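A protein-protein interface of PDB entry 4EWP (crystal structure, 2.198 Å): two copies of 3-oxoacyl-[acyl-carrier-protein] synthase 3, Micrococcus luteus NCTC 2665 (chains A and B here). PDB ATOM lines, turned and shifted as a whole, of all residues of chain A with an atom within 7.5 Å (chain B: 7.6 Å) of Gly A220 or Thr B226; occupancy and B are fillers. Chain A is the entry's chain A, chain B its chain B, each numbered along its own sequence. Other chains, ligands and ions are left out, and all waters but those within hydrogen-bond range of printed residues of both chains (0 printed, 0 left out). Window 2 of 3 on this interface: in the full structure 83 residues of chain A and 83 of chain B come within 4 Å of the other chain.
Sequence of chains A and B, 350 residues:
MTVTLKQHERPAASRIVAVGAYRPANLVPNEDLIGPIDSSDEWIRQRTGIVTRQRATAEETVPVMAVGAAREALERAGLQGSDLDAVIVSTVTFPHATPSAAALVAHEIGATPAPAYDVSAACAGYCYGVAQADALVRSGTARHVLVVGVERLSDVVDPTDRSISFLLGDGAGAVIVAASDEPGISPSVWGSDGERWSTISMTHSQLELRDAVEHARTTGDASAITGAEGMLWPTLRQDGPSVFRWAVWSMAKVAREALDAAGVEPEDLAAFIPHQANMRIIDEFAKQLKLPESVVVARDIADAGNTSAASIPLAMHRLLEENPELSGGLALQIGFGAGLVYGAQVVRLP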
ATOM      1  N   VAL A 213     -19.352   2.039   6.030  1.00  0.00           N
ATOM      2  CA  VAL A 213     -20.545   1.409   6.590  1.00  0.00           C
ATOM      3  C   VAL A 213     -21.668   1.311   5.569  1.00  0.00           C
ATOM      4  O   VAL A 213     -22.353   0.291   5.485  1.00  0.00           O
ATOM      5  CB  VAL A 213     -21.058   2.143   7.854  1.00  0.00           C
ATOM      6  CG1 VAL A 213     -21.620   3.517   7.495  1.00  0.00           C
ATOM      7  CG2 VAL A 213     -22.118   1.309   8.555  1.00  0.00           C
ATOM      8  N   GLU A 214     -21.852   2.360   4.775  1.00  0.00           N
ATOM      9  CA  GLU A 214     -22.945   2.352   3.808  1.00  0.00           C
ATOM     10  C   GLU A 214     -22.623   1.517   2.574  1.00  0.00           C
ATOM     11  O   GLU A 214     -23.526   0.941   1.966  1.00  0.00           O
ATOM     12  CB  GLU A 214     -23.400   3.772   3.446  1.00  0.00           C
ATOM     13  CG  GLU A 214     -24.041   4.546   4.631  1.00  0.00           C
ATOM     14  CD  GLU A 214     -25.297   3.871   5.195  1.00  0.00           C
ATOM     15  OE1 GLU A 214     -26.137   3.405   4.399  1.00  0.00           O
ATOM     16  OE2 GLU A 214     -25.443   3.808   6.435  1.00  0.00           O
ATOM     17  N   HIS A 215     -21.343   1.441   2.209  1.00  0.00           N
ATOM     18  CA  HIS A 215     -20.916   0.557   1.119  1.00  0.00           C
ATOM     19  C   HIS A 215     -21.089  -0.891   1.555  1.00  0.00           C
ATOM     20  O   HIS A 215     -21.521  -1.741   0.780  1.00  0.00           O
ATOM     21  CB  HIS A 215     -19.460   0.816   0.723  1.00  0.00           C
ATOM     22  CG  HIS A 215     -18.954  -0.078  -0.371  1.00  0.00           C
ATOM     23  ND1 HIS A 215     -18.386  -1.311  -0.125  1.00  0.00           N
ATOM     24  CD2 HIS A 215     -18.913   0.092  -1.715  1.00  0.00           C
ATOM     25  CE1 HIS A 215     -18.027  -1.867  -1.269  1.00  0.00           C
ATOM     26  NE2 HIS A 215     -18.335  -1.036  -2.249  1.00  0.00           N
ATOM     27  N   ALA A 216     -20.757  -1.162   2.812  1.00  0.00           N
ATOM     28  CA  ALA A 216     -20.957  -2.492   3.371  1.00  0.00           C
ATOM     29  C   ALA A 216     -22.442  -2.827   3.374  1.00  0.00           C
ATOM     30  O   ALA A 216     -22.859  -3.892   2.908  1.00  0.00           O
ATOM     31  CB  ALA A 216     -20.393  -2.560   4.777  1.00  0.00           C
ATOM     32  N   ARG A 217     -23.236  -1.899   3.893  1.00  0.00           N
ATOM     33  CA  ARG A 217     -24.679  -2.082   3.989  1.00  0.00           C
ATOM     34  C   ARG A 217     -25.353  -2.334   2.639  1.00  0.00           C
ATOM     35  O   ARG A 217     -26.152  -3.253   2.514  1.00  0.00           O
ATOM     36  CB  ARG A 217     -25.333  -0.888   4.687  1.00  0.00           C
ATOM     37  CG  ARG A 217     -26.757  -1.160   5.135  1.00  0.00           C
ATOM     38  CD  ARG A 217     -27.404   0.088   5.707  1.00  0.00           C
ATOM     39  NE  ARG A 217     -27.558   1.103   4.668  1.00  0.00           N
ATOM     40  CZ  ARG A 217     -28.605   1.184   3.850  1.00  0.00           C
ATOM     41  NH1 ARG A 217     -29.605   0.312   3.953  1.00  0.00           N
ATOM     42  NH2 ARG A 217     -28.654   2.136   2.924  1.00  0.00           N
ATOM     43  N   THR A 218     -25.042  -1.518   1.637  1.00  0.00           N
ATOM     44  CA  THR A 218     -25.654  -1.694   0.317  1.00  0.00           C
ATOM     45  C   THR A 218     -25.200  -2.974  -0.395  1.00  0.00           C
ATOM     46  O   THR A 218     -26.027  -3.774  -0.833  1.00  0.00           O
ATOM     47  CB  THR A 218     -25.476  -0.453  -0.614  1.00  0.00           C
ATOM     48  OG1 THR A 218     -24.096  -0.071  -0.692  1.00  0.00           O
ATOM     49  CG2 THR A 218     -26.291   0.727  -0.111  1.00  0.00           C
ATOM     50  N   THR A 219     -23.888  -3.176  -0.498  1.00  0.00           N
ATOM     51  CA  THR A 219     -23.346  -4.281  -1.300  1.00  0.00           C
ATOM     52  C   THR A 219     -23.297  -5.641  -0.595  1.00  0.00           C
ATOM     53  O   THR A 219     -23.034  -6.663  -1.237  1.00  0.00           O
ATOM     54  CB  THR A 219     -21.929  -3.970  -1.820  1.00  0.00           C
ATOM     55  OG1 THR A 219     -21.024  -3.895  -0.712  1.00  0.00           O
ATOM     56  CG2 THR A 219     -21.909  -2.657  -2.588  1.00  0.00           C
ATOM     57  N   GLY A 220     -23.536  -5.653   0.713  1.00  0.00           N
ATOM     58  CA  GLY A 220     -23.462  -6.881   1.488  1.00  0.00           C
ATOM     59  C   GLY A 220     -22.037  -7.354   1.747  1.00  0.00           C
ATOM     60  O   GLY A 220     -21.829  -8.323   2.479  1.00  0.00           O
ATOM     61  N   ASP A 221     -21.058  -6.680   1.145  1.00  0.00           N
ATOM     62  CA  ASP A 221     -19.644  -6.980   1.381  1.00  0.00           C
ATOM     63  C   ASP A 221     -19.086  -6.150   2.532  1.00  0.00           C
ATOM     64  O   ASP A 221     -18.819  -4.959   2.377  1.00  0.00           O
ATOM     65  CB  ASP A 221     -18.816  -6.713   0.124  1.00  0.00           C
ATOM     66  CG  ASP A 221     -17.320  -6.717   0.400  1.00  0.00           C
ATOM     67  OD1 ASP A 221     -16.892  -7.338   1.399  1.00  0.00           O
ATOM     68  OD2 ASP A 221     -16.568  -6.099  -0.383  1.00  0.00           O
ATOM     69  N   ALA A 222     -18.890  -6.781   3.681  1.00  0.00           N
ATOM     70  CA  ALA A 222     -18.415  -6.051   4.847  1.00  0.00           C
ATOM     71  C   ALA A 222     -16.942  -6.274   5.141  1.00  0.00           C
ATOM     72  O   ALA A 222     -16.504  -6.101   6.275  1.00  0.00           O
ATOM     73  CB  ALA A 222     -19.261  -6.387   6.078  1.00  0.00           C
ATOM     74  N   SER A 223     -16.170  -6.648   4.129  1.00  0.00           N
ATOM     75  CA  SER A 223     -14.721  -6.613   4.271  1.00  0.00           C
ATOM     76  C   SER A 223     -14.394  -5.156   4.583  1.00  0.00           C
ATOM     77  O   SER A 223     -15.300  -4.365   4.867  1.00  0.00           O
ATOM     78  CB  SER A 223     -14.017  -7.091   2.993  1.00  0.00           C
ATOM     79  OG  SER A 223     -14.162  -6.167   1.931  1.00  0.00           O
ATOM     80  N   ASP B 221     -18.301 -10.517  12.992  1.00  0.00           N
ATOM     81  CA  ASP B 221     -19.727 -10.657  12.737  1.00  0.00           C
ATOM     82  C   ASP B 221     -20.268  -9.332  12.233  1.00  0.00           C
ATOM     83  O   ASP B 221     -20.477  -8.402  13.008  1.00  0.00           O
ATOM     84  CB  ASP B 221     -20.468 -11.086  14.003  1.00  0.00           C
ATOM     85  CG  ASP B 221     -21.969 -11.190  13.793  1.00  0.00           C
ATOM     86  OD1 ASP B 221     -22.422 -11.017  12.637  1.00  0.00           O
ATOM     87  OD2 ASP B 221     -22.694 -11.452  14.779  1.00  0.00           O
ATOM     88  N   ALA B 222     -20.502  -9.242  10.931  1.00  0.00           N
ATOM     89  CA  ALA B 222     -20.892  -7.968  10.350  1.00  0.00           C
ATOM     90  C   ALA B 222     -22.391  -7.873  10.102  1.00  0.00           C
ATOM     91  O   ALA B 222     -22.852  -6.958   9.421  1.00  0.00           O
ATOM     92  CB  ALA B 222     -20.127  -7.714   9.068  1.00  0.00           C
ATOM     93  N   SER B 223     -23.153  -8.815  10.648  1.00  0.00           N
ATOM     94  CA  SER B 223     -24.600  -8.670  10.673  1.00  0.00           C
ATOM     95  C   SER B 223     -24.897  -7.312  11.272  1.00  0.00           C
ATOM     96  O   SER B 223     -24.008  -6.677  11.848  1.00  0.00           O
ATOM     97  CB  SER B 223     -25.235  -9.742  11.546  1.00  0.00           C
ATOM     98  OG  SER B 223     -24.761 -11.010  11.199  1.00  0.00           O
ATOM     99  N   ALA B 224     -26.145  -6.874  11.159  1.00  0.00           N
ATOM    100  CA  ALA B 224     -26.545  -5.567  11.674  1.00  0.00           C
ATOM    101  C   ALA B 224     -26.021  -4.447  10.796  1.00  0.00           C
ATOM    102  O   ALA B 224     -26.559  -3.351  10.815  1.00  0.00           O
ATOM    103  CB  ALA B 224     -26.082  -5.377  13.115  1.00  0.00           C
ATOM    104  N   ILE B 225     -24.976  -4.717  10.022  1.00  0.00           N
ATOM    105  CA  ILE B 225     -24.547  -3.757   9.013  1.00  0.00           C
ATOM    106  C   ILE B 225     -25.033  -4.182   7.627  1.00  0.00           C
ATOM    107  O   ILE B 225     -25.749  -3.432   6.972  1.00  0.00           O
ATOM    108  CB  ILE B 225     -23.034  -3.516   9.025  1.00  0.00           C
ATOM    109  CG1 ILE B 225     -22.612  -2.967  10.390  1.00  0.00           C
ATOM    110  CG2 ILE B 225     -22.655  -2.539   7.922  1.00  0.00           C
ATOM    111  CD1 ILE B 225     -21.164  -2.558  10.472  1.00  0.00           C
ATOM    112  N   THR B 226     -24.647  -5.376   7.179  1.00  0.00           N
ATOM    113  CA  THR B 226     -25.302  -5.980   6.019  1.00  0.00           C
ATOM    114  C   THR B 226     -26.681  -6.413   6.498  1.00  0.00           C
ATOM    115  O   THR B 226     -26.831  -6.877   7.633  1.00  0.00           O
ATOM    116  CB  THR B 226     -24.542  -7.214   5.462  1.00  0.00           C
ATOM    117  OG1 THR B 226     -24.520  -8.262   6.443  1.00  0.00           O
ATOM    118  CG2 THR B 226     -23.113  -6.849   5.071  1.00  0.00           C
ATOM    119  N   GLY B 227     -27.695  -6.249   5.662  1.00  0.00           N
ATOM    120  CA  GLY B 227     -29.037  -6.594   6.087  1.00  0.00           C
ATOM    121  C   GLY B 227     -29.579  -5.642   7.139  1.00  0.00           C
ATOM    122  O   GLY B 227     -30.518  -5.969   7.870  1.00  0.00           O
ATOM    123  N   ALA B 228     -28.976  -4.461   7.233  1.00  0.00           N
ATOM    124  CA  ALA B 228     -29.600  -3.375   7.966  1.00  0.00           C
ATOM    125  C   ALA B 228     -30.514  -2.675   6.980  1.00  0.00           C
ATOM    126  O   ALA B 228     -30.071  -2.220   5.924  1.00  0.00           O
ATOM    127  CB  ALA B 228     -28.564  -2.413   8.505  1.00  0.00           C
ATOM    128  N   GLU B 229     -31.798  -2.633   7.298  1.00  0.00           N
ATOM    129  CA  GLU B 229     -32.724  -1.841   6.516  1.00  0.00           C
ATOM    130  C   GLU B 229     -32.609  -0.418   7.029  1.00  0.00           C
ATOM    131  O   GLU B 229     -32.810  -0.158   8.218  1.00  0.00           O
ATOM    132  CB  GLU B 229     -34.140  -2.366   6.696  1.00  0.00           C
ATOM    133  CG  GLU B 229     -34.376  -2.963   8.066  1.00  0.00           C
ATOM    134  CD  GLU B 229     -35.097  -4.292   7.994  1.00  0.00           C
ATOM    135  OE1 GLU B 229     -36.342  -4.278   7.876  1.00  0.00           O
ATOM    136  OE2 GLU B 229     -34.423  -5.347   8.049  1.00  0.00           O
ATOM    137  N   LEU B 232     -27.243   3.350   8.588  1.00  0.00           N
ATOM    138  CA  LEU B 232     -26.579   3.380   9.881  1.00  0.00           C
ATOM    139  C   LEU B 232     -25.964   4.764  10.086  1.00  0.00           C
ATOM    140  O   LEU B 232     -25.907   5.283  11.201  1.00  0.00           O
ATOM    141  CB  LEU B 232     -25.487   2.315   9.939  1.00  0.00           C
ATOM    142  CG  LEU B 232     -25.856   0.871  10.285  1.00  0.00           C
ATOM    143  CD1 LEU B 232     -27.350   0.711  10.523  1.00  0.00           C
ATOM    144  CD2 LEU B 232     -25.365  -0.092   9.203  1.00  0.00           C
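NH1 of Arg A217 sits at hydrogen-bond distance from O of Ala B228 (3.2 Å).
The side-chain carboxylate (OE2) of Glu A214 is in hydrogen-bond range of the backbone NH (N) of Leu B232 (2.8 Å).
The guanidinium group of Arg A217 lies within salt-bridge range of the side-chain carboxylate of Glu A214 (2.7 Å).
The backbone carbonyl oxygen of Glu A214 sits at hydrogen-bond distance from the side-chain hydroxyl of Thr A218 (2.9 Å).
Val A213 touches Ile B225.
CD2 of Leu B232 touches CG2 of Val A213, 3.6 Å away.
CG2 of Ile B225 touches CB of Ala A216, 3.9 Å away.
Ala A216 touches Thr B226.
O of Ile B225 touches CG of Arg A217, 3.1 Å away.
Gly A220 touches Thr B226 (O to CG2, 3.2 Å).
CB of Ala A222 touches CB of Ala B222, 3.4 Å away.
Printed residues of chain B within 4 Å of Glu A214: Leu B232 (2.8 Å).
Printed residues of chain B within 4 Å of Ala A216: Ile B225 (3.9 Å) and Thr B226 (3.7 Å).
Of the printed residues of chain B, Ala A222 touches Ala B222 (3.4 Å).
Of the printed residues of chain A, Ala B222 touches Ala A222 (3.4 Å).
Of the printed residues of chain A, Thr B226 touches Ala A216 (3.7 Å) and Gly A220 (3.2 Å).
Printed residues of chain A within 4 Å of Leu B232: Val A213 (3.6 Å) and Glu A214 (2.8 Å).
The nearest printed residue of chain A that does not touch Thr B226 is Ala A222 (4.01 Å).
The nearest printed residue of chain A that does not touch Leu B232 is Arg A217 (4.1 Å).
Along chain A the printed residues that touch a printed residue of chain B span positions 213 to 222.
Among the printed residues, 9 pairs touch across the chains.
Among the printed residues, no Asp or Glu carboxylate lies within 4 Å of a Lys or Arg side-chain nitrogen of the other chain.
Ala A222 touches its own counterpart, Ala B222.
3 positions are printed for both chains.
Of the 9 pairs that touch across the chains among the printed residues, 1 has its exchanged pair printed and touching as well.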
